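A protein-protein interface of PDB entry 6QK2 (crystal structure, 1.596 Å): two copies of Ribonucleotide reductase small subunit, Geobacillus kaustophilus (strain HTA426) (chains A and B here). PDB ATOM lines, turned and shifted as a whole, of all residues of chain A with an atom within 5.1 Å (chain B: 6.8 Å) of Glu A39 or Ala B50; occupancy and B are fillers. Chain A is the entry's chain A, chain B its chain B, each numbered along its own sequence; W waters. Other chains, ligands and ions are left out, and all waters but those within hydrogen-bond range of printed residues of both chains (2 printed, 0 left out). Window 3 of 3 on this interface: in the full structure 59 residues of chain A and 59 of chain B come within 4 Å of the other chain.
Glu A39 touches just these residues of chain B: Ala B50 (3.4 Å), Glu B121 (2.9 Å) and Arg B125 (3.1 Å).
Ala B50 touches just these residues of chain A: Glu A39 and Arg A43.
Of the printed residues of chain B, Lys A42 touches Asn B48 and Glu B121.
Of the printed residues of chain A, Glu B121 touches Tyr A38, Glu A39 and Lys A42.
Of the printed residues of chain A, Asn B48 touches Lys A42 (2.8 Å) and Arg A43 (3.7 Å).
Of the printed residues of chain B, Phe A35 touches Arg B125.
The nearest residue of chain B that does not touch Glu A39 is Asn B48 (4.6 Å).
Hydrophobic or aromatic side chains of chain A within 4 Å of the printed part of chain B: Phe A35 and Tyr A38.
Along chain A the printed residues that touch a printed residue of chain B span positions 35 to 43.
Printed residues of chain B that touch a printed residue of chain A: Asn B48, Ala B50, Asp B51, Glu B121 and Arg B125.
Among the printed residues, 10 pairs touch across the chains.
Among the printed residues, Asp or Glu carboxylates within 4 Å of a Lys or Arg side-chain nitrogen of the other chain: Glu A39 with Arg B125, Lys A42 with Glu B121 and Arg A43 with Asp B51.
Water W1 lies within hydrogen-bond range of OE1 of Glu A39 (2.8 Å), ND2 of Asn B48 (3.0 Å) and NE of Arg A43 (3.4 Å).
Water W2 bridges the side-chain amide nitrogen of Asn B48 and the guanidinium group of Arg A43.
The side-chain carboxylate (OE2) of Glu A39 lies close to the side-chain carboxylate (OE1) of Glu B121 (2.9 Å).
The side-chain carboxylate (OD1) of Asp B51 lies within salt-bridge range of the guanidinium group (NH2) of Arg A43 (2.5 Å).
The side-chain carboxylate (OE2) of Glu A39 is in salt-bridge range of the guanidinium group (NH2) of Arg B125 (3.1 Å).
The side-chain carboxylate of Glu B121 lies within salt-bridge range of the side-chain amino group of Lys A42.
The side-chain amino group (NZ) of Lys A42 lies within hydrogen-bond range of the side-chain amide oxygen (OD1) of Asn B48 (2.8 Å).
The side-chain hydroxyl (OH) of Tyr A38 is in hydrogen-bond range of the side-chain carboxylate (OE2) of Glu B121 (2.7 Å).
The side-chain carboxylate of Glu B121 lies within salt-bridge range of the guanidinium group of Arg B125, at 2.7 Å.
OD1 of Asn B48 is in hydrogen-bond range of N of Ala B50 (2.9 Å).
The side-chain amino group of Lys A42 is in salt-bridge range of the side-chain carboxylate of Glu A39 (2.7 Å).
Arg B125 touches Phe A35 (NH2 to CZ, 3.8 Å).
Glu A39 touches Ala B50 (OE1 to CB, 3.4 Å).
CZ of Arg A43 touches ND2 of Asn B48 (3.7 Å).
Arg A43 touches Ala B50 (NH2 to CB, 3.8 Å).
No position is printed for both chains.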
ATOM      1  N   MET A  34      -6.651  24.654 -21.153  1.00  0.00           N
ATOM      2  CA  MET A  34      -5.847  24.725 -19.942  1.00  0.00           C
ATOM      3  C   MET A  34      -6.668  25.066 -18.726  1.00  0.00           C
ATOM      4  O   MET A  34      -6.276  24.682 -17.625  1.00  0.00           O
ATOM      5  CB  MET A  34      -4.700  25.704 -20.117  1.00  0.00           C
ATOM      6  CG  MET A  34      -3.730  25.224 -21.216  1.00  0.00           C
ATOM      7  SD  MET A  34      -2.924  23.603 -20.886  1.00  0.00           S
ATOM      8  CE  MET A  34      -3.921  22.498 -21.856  1.00  0.00           C
ATOM      9  N   PHE A  35      -7.841  25.710 -18.877  1.00  0.00           N
ATOM     10  CA  PHE A  35      -8.713  25.817 -17.711  1.00  0.00           C
ATOM     11  C   PHE A  35      -9.283  24.455 -17.316  1.00  0.00           C
ATOM     12  O   PHE A  35      -9.380  24.132 -16.123  1.00  0.00           O
ATOM     13  CB  PHE A  35      -9.859  26.820 -17.946  1.00  0.00           C
ATOM     14  CG  PHE A  35     -10.673  27.047 -16.703  1.00  0.00           C
ATOM     15  CD1 PHE A  35     -10.141  27.789 -15.665  1.00  0.00           C
ATOM     16  CD2 PHE A  35     -11.911  26.444 -16.529  1.00  0.00           C
ATOM     17  CE1 PHE A  35     -10.836  27.959 -14.478  1.00  0.00           C
ATOM     18  CE2 PHE A  35     -12.620  26.617 -15.330  1.00  0.00           C
ATOM     19  CZ  PHE A  35     -12.059  27.377 -14.311  1.00  0.00           C
ATOM     20  N   LYS A  36      -9.696  23.649 -18.295  1.00  0.00           N
ATOM     21  CA  LYS A  36     -10.194  22.316 -17.996  1.00  0.00           C
ATOM     22  C   LYS A  36      -9.100  21.468 -17.346  1.00  0.00           C
ATOM     23  O   LYS A  36      -9.364  20.741 -16.378  1.00  0.00           O
ATOM     24  CB  LYS A  36     -10.730  21.688 -19.277  1.00  0.00           C
ATOM     25  CG  LYS A  36     -11.929  22.473 -19.801  1.00  0.00           C
ATOM     26  CD  LYS A  36     -12.738  21.663 -20.765  1.00  0.00           C
ATOM     27  CE  LYS A  36     -14.165  22.212 -20.863  1.00  0.00           C
ATOM     28  NZ  LYS A  36     -14.918  22.109 -19.577  1.00  0.00           N
ATOM     29  N   LEU A  37      -7.846  21.624 -17.801  1.00  0.00           N
ATOM     30  CA  LEU A  37      -6.738  20.884 -17.187  1.00  0.00           C
ATOM     31  C   LEU A  37      -6.474  21.363 -15.756  1.00  0.00           C
ATOM     32  O   LEU A  37      -6.191  20.559 -14.868  1.00  0.00           O
ATOM     33  CB  LEU A  37      -5.486  21.023 -18.063  1.00  0.00           C
ATOM     34  CG  LEU A  37      -4.341  20.028 -17.805  1.00  0.00           C
ATOM     35  CD1 LEU A  37      -4.823  18.602 -18.131  1.00  0.00           C
ATOM     36  CD2 LEU A  37      -3.117  20.380 -18.649  1.00  0.00           C
ATOM     37  N   TYR A  38      -6.563  22.678 -15.522  1.00  0.00           N
ATOM     38  CA  TYR A  38      -6.474  23.250 -14.183  1.00  0.00           C
ATOM     39  C   TYR A  38      -7.543  22.671 -13.258  1.00  0.00           C
ATOM     40  O   TYR A  38      -7.281  22.351 -12.091  1.00  0.00           O
ATOM     41  CB  TYR A  38      -6.602  24.769 -14.309  1.00  0.00           C
ATOM     42  CG  TYR A  38      -6.936  25.560 -13.065  1.00  0.00           C
ATOM     43  CD1 TYR A  38      -5.981  25.814 -12.087  1.00  0.00           C
ATOM     44  CD2 TYR A  38      -8.198  26.112 -12.882  1.00  0.00           C
ATOM     45  CE1 TYR A  38      -6.275  26.593 -10.964  1.00  0.00           C
ATOM     46  CE2 TYR A  38      -8.490  26.870 -11.745  1.00  0.00           C
ATOM     47  CZ  TYR A  38      -7.534  27.112 -10.807  1.00  0.00           C
ATOM     48  OH  TYR A  38      -7.841  27.871  -9.678  1.00  0.00           O
ATOM     49  N   GLU A  39      -8.768  22.539 -13.763  1.00  0.00           N
ATOM     50  CA  GLU A  39      -9.833  21.986 -12.949  1.00  0.00           C
ATOM     51  C   GLU A  39      -9.552  20.538 -12.585  1.00  0.00           C
ATOM     52  O   GLU A  39      -9.764  20.138 -11.438  1.00  0.00           O
ATOM     53  CB  GLU A  39     -11.170  22.142 -13.688  1.00  0.00           C
ATOM     54  CG  GLU A  39     -11.675  23.607 -13.750  1.00  0.00           C
ATOM     55  CD  GLU A  39     -12.186  24.124 -12.393  1.00  0.00           C
ATOM     56  OE1 GLU A  39     -12.955  23.423 -11.730  1.00  0.00           O
ATOM     57  OE2 GLU A  39     -11.793  25.225 -11.967  1.00  0.00           O
ATOM     58  N   LYS A  40      -9.070  19.749 -13.541  1.00  0.00           N
ATOM     59  CA  LYS A  40      -8.679  18.364 -13.268  1.00  0.00           C
ATOM     60  C   LYS A  40      -7.552  18.305 -12.251  1.00  0.00           C
ATOM     61  O   LYS A  40      -7.526  17.430 -11.370  1.00  0.00           O
ATOM     62  CB  LYS A  40      -8.224  17.679 -14.568  1.00  0.00           C
ATOM     63  CG  LYS A  40      -9.321  17.438 -15.596  1.00  0.00           C
ATOM     64  CD  LYS A  40      -8.876  16.429 -16.681  1.00  0.00           C
ATOM     65  CE  LYS A  40      -8.213  17.116 -17.892  1.00  0.00           C
ATOM     66  NZ  LYS A  40      -7.465  16.153 -18.791  1.00  0.00           N
ATOM     67  N   ALA A  41      -6.603  19.235 -12.348  1.00  0.00           N
ATOM     68  CA  ALA A  41      -5.470  19.231 -11.438  1.00  0.00           C
ATOM     69  C   ALA A  41      -5.921  19.451 -10.005  1.00  0.00           C
ATOM     70  O   ALA A  41      -5.409  18.812  -9.079  1.00  0.00           O
ATOM     71  CB  ALA A  41      -4.465  20.299 -11.840  1.00  0.00           C
ATOM     72  N   LYS A  42      -6.889  20.344  -9.790  1.00  0.00           N
ATOM     73  CA  LYS A  42      -7.392  20.549  -8.434  1.00  0.00           C
ATOM     74  C   LYS A  42      -8.110  19.308  -7.916  1.00  0.00           C
ATOM     75  O   LYS A  42      -7.923  18.920  -6.753  1.00  0.00           O
ATOM     76  CB  LYS A  42      -8.343  21.737  -8.388  1.00  0.00           C
ATOM     77  CG  LYS A  42      -7.687  23.097  -8.593  1.00  0.00           C
ATOM     78  CD  LYS A  42      -8.743  24.220  -8.507  1.00  0.00           C
ATOM     79  CE  LYS A  42      -9.628  24.239  -9.714  1.00  0.00           C
ATOM     80  NZ  LYS A  42     -10.833  25.092  -9.458  1.00  0.00           N
ATOM     81  N   ARG A  43      -8.947  18.684  -8.761  1.00  0.00           N
ATOM     82  CA  ARG A  43      -9.712  17.504  -8.353  1.00  0.00           C
ATOM     83  C   ARG A  43      -8.793  16.332  -8.034  1.00  0.00           C
ATOM     84  O   ARG A  43      -9.036  15.586  -7.075  1.00  0.00           O
ATOM     85  CB  ARG A  43     -10.697  17.099  -9.450  1.00  0.00           C
ATOM     86  CG  ARG A  43     -11.842  18.061  -9.686  1.00  0.00           C
ATOM     87  CD  ARG A  43     -12.811  18.106  -8.522  1.00  0.00           C
ATOM     88  NE  ARG A  43     -13.888  19.082  -8.728  1.00  0.00           N
ATOM     89  CZ  ARG A  43     -14.644  19.572  -7.750  1.00  0.00           C
ATOM     90  NH1 ARG A  43     -14.434  19.198  -6.495  1.00  0.00           N
ATOM     91  NH2 ARG A  43     -15.594  20.467  -8.019  1.00  0.00           N
ATOM     92  N   TRP B  47      -9.645  23.693  -0.242  1.00  0.00           N
ATOM     93  CA  TRP B  47     -10.891  24.216  -0.790  1.00  0.00           C
ATOM     94  C   TRP B  47     -10.796  24.452  -2.296  1.00  0.00           C
ATOM     95  O   TRP B  47      -9.730  24.739  -2.852  1.00  0.00           O
ATOM     96  CB  TRP B  47     -11.273  25.504  -0.058  1.00  0.00           C
ATOM     97  CG  TRP B  47     -10.547  26.737  -0.496  1.00  0.00           C
ATOM     98  CD1 TRP B  47      -9.281  27.104  -0.151  1.00  0.00           C
ATOM     99  CD2 TRP B  47     -11.063  27.787  -1.327  1.00  0.00           C
ATOM    100  NE1 TRP B  47      -8.968  28.320  -0.718  1.00  0.00           N
ATOM    101  CE2 TRP B  47     -10.033  28.750  -1.466  1.00  0.00           C
ATOM    102  CE3 TRP B  47     -12.284  27.997  -1.983  1.00  0.00           C
ATOM    103  CZ2 TRP B  47     -10.202  29.920  -2.194  1.00  0.00           C
ATOM    104  CZ3 TRP B  47     -12.451  29.151  -2.724  1.00  0.00           C
ATOM    105  CH2 TRP B  47     -11.409  30.103  -2.824  1.00  0.00           C
ATOM    106  N   ASN B  48     -11.949  24.353  -2.954  1.00  0.00           N
ATOM    107  CA  ASN B  48     -12.036  24.466  -4.406  1.00  0.00           C
ATOM    108  C   ASN B  48     -13.164  25.426  -4.736  1.00  0.00           C
ATOM    109  O   ASN B  48     -14.327  25.151  -4.370  1.00  0.00           O
ATOM    110  CB  ASN B  48     -12.275  23.101  -5.048  1.00  0.00           C
ATOM    111  CG  ASN B  48     -12.157  23.132  -6.552  1.00  0.00           C
ATOM    112  OD1 ASN B  48     -12.297  24.171  -7.196  1.00  0.00           O
ATOM    113  ND2 ASN B  48     -11.912  21.974  -7.131  1.00  0.00           N
ATOM    114  N   PRO B  49     -12.891  26.548  -5.420  1.00  0.00           N
ATOM    115  CA  PRO B  49     -13.979  27.453  -5.817  1.00  0.00           C
ATOM    116  C   PRO B  49     -15.067  26.800  -6.642  1.00  0.00           C
ATOM    117  O   PRO B  49     -16.212  27.289  -6.635  1.00  0.00           O
ATOM    118  CB  PRO B  49     -13.261  28.522  -6.640  1.00  0.00           C
ATOM    119  CG  PRO B  49     -11.817  28.425  -6.295  1.00  0.00           C
ATOM    120  CD  PRO B  49     -11.550  27.090  -5.730  1.00  0.00           C
ATOM    121  N   ALA B  50     -14.734  25.743  -7.381  1.00  0.00           N
ATOM    122  CA  ALA B  50     -15.716  25.041  -8.199  1.00  0.00           C
ATOM    123  C   ALA B  50     -16.776  24.339  -7.358  1.00  0.00           C
ATOM    124  O   ALA B  50     -17.826  23.986  -7.901  1.00  0.00           O
ATOM    125  CB  ALA B  50     -15.023  24.030  -9.100  1.00  0.00           C
ATOM    126  N   ASP B  51     -16.580  24.206  -6.049  1.00  0.00           N
ATOM    127  CA  ASP B  51     -17.569  23.554  -5.192  1.00  0.00           C
ATOM    128  C   ASP B  51     -18.529  24.534  -4.521  1.00  0.00           C
ATOM    129  O   ASP B  51     -19.468  24.091  -3.850  1.00  0.00           O
ATOM    130  CB  ASP B  51     -16.893  22.728  -4.081  1.00  0.00           C
ATOM    131  CG  ASP B  51     -16.025  21.587  -4.612  1.00  0.00           C
ATOM    132  OD1 ASP B  51     -16.329  21.065  -5.704  1.00  0.00           O
ATOM    133  OD2 ASP B  51     -15.045  21.214  -3.912  1.00  0.00           O
ATOM    134  N   ILE B  52     -18.301  25.842  -4.638  1.00  0.00           N
ATOM    135  CA  ILE B  52     -19.174  26.817  -3.990  1.00  0.00           C
ATOM    136  C   ILE B  52     -20.485  26.893  -4.759  1.00  0.00           C
ATOM    137  O   ILE B  52     -20.508  27.010  -5.992  1.00  0.00           O
ATOM    138  CB  ILE B  52     -18.504  28.194  -3.910  1.00  0.00           C
ATOM    139  CG1 ILE B  52     -17.287  28.150  -2.997  1.00  0.00           C
ATOM    140  CG2 ILE B  52     -19.500  29.272  -3.391  1.00  0.00           C
ATOM    141  CD1 ILE B  52     -16.474  29.404  -3.018  1.00  0.00           C
ATOM    142  N   ASP B  53     -21.588  26.836  -4.024  1.00  0.00           N
ATOM    143  CA  ASP B  53     -22.925  26.986  -4.594  1.00  0.00           C
ATOM    144  C   ASP B  53     -23.263  28.476  -4.654  1.00  0.00           C
ATOM    145  O   ASP B  53     -23.412  29.126  -3.617  1.00  0.00           O
ATOM    146  CB  ASP B  53     -23.901  26.198  -3.723  1.00  0.00           C
ATOM    147  CG  ASP B  53     -25.328  26.293  -4.188  1.00  0.00           C
ATOM    148  OD1 ASP B  53     -25.614  26.997  -5.176  1.00  0.00           O
ATOM    149  OD2 ASP B  53     -26.171  25.639  -3.535  1.00  0.00           O
ATOM    150  N   PHE B  54     -23.312  29.030  -5.870  1.00  0.00           N
ATOM    151  CA  PHE B  54     -23.646  30.432  -6.079  1.00  0.00           C
ATOM    152  C   PHE B  54     -25.118  30.606  -6.472  1.00  0.00           C
ATOM    153  O   PHE B  54     -25.503  31.690  -6.916  1.00  0.00           O
ATOM    154  CB  PHE B  54     -22.753  31.051  -7.164  1.00  0.00           C
ATOM    155  CG  PHE B  54     -21.305  31.235  -6.764  1.00  0.00           C
ATOM    156  CD1 PHE B  54     -20.311  30.482  -7.368  1.00  0.00           C
ATOM    157  CD2 PHE B  54     -20.944  32.190  -5.837  1.00  0.00           C
ATOM    158  CE1 PHE B  54     -18.974  30.654  -7.023  1.00  0.00           C
ATOM    159  CE2 PHE B  54     -19.595  32.385  -5.497  1.00  0.00           C
ATOM    160  CZ  PHE B  54     -18.617  31.601  -6.108  1.00  0.00           C
ATOM    161  N   GLU B 121     -10.217  32.829  -9.644  1.00  0.00           N
ATOM    162  CA  GLU B 121     -11.295  31.975 -10.092  1.00  0.00           C
ATOM    163  C   GLU B 121     -12.559  32.229  -9.303  1.00  0.00           C
ATOM    164  O   GLU B 121     -13.654  32.259  -9.881  1.00  0.00           O
ATOM    165  CB  GLU B 121     -10.868  30.509  -9.945  1.00  0.00           C
ATOM    166  CG  GLU B 121     -11.927  29.543 -10.400  1.00  0.00           C
ATOM    167  CD  GLU B 121     -11.641  28.122  -9.961  1.00  0.00           C
ATOM    168  OE1 GLU B 121     -12.535  27.290 -10.141  1.00  0.00           O
ATOM    169  OE2 GLU B 121     -10.516  27.836  -9.448  1.00  0.00           O
ATOM    170  N   ARG B 125     -15.975  33.342 -11.045  1.00  0.00           N
ATOM    171  CA  ARG B 125     -17.124  32.453 -10.987  1.00  0.00           C
ATOM    172  C   ARG B 125     -18.341  33.194 -10.467  1.00  0.00           C
ATOM    173  O   ARG B 125     -19.457  32.963 -10.947  1.00  0.00           O
ATOM    174  CB  ARG B 125     -16.864  31.233 -10.093  1.00  0.00           C
ATOM    175  CG  ARG B 125     -16.058  30.146 -10.791  1.00  0.00           C
ATOM    176  CD  ARG B 125     -15.895  28.925  -9.877  1.00  0.00           C
ATOM    177  NE  ARG B 125     -15.117  27.883 -10.543  1.00  0.00           N
ATOM    178  CZ  ARG B 125     -15.574  27.041 -11.467  1.00  0.00           C
ATOM    179  NH1 ARG B 125     -16.835  27.077 -11.859  1.00  0.00           N
ATOM    180  NH2 ARG B 125     -14.764  26.148 -12.011  1.00  0.00           N
HETATM  181  O   HOH W   1     -11.900  21.501 -10.051  1.00  0.00           O
HETATM  182  O   HOH W   2     -11.243  19.596  -5.459  1.00  0.00           O
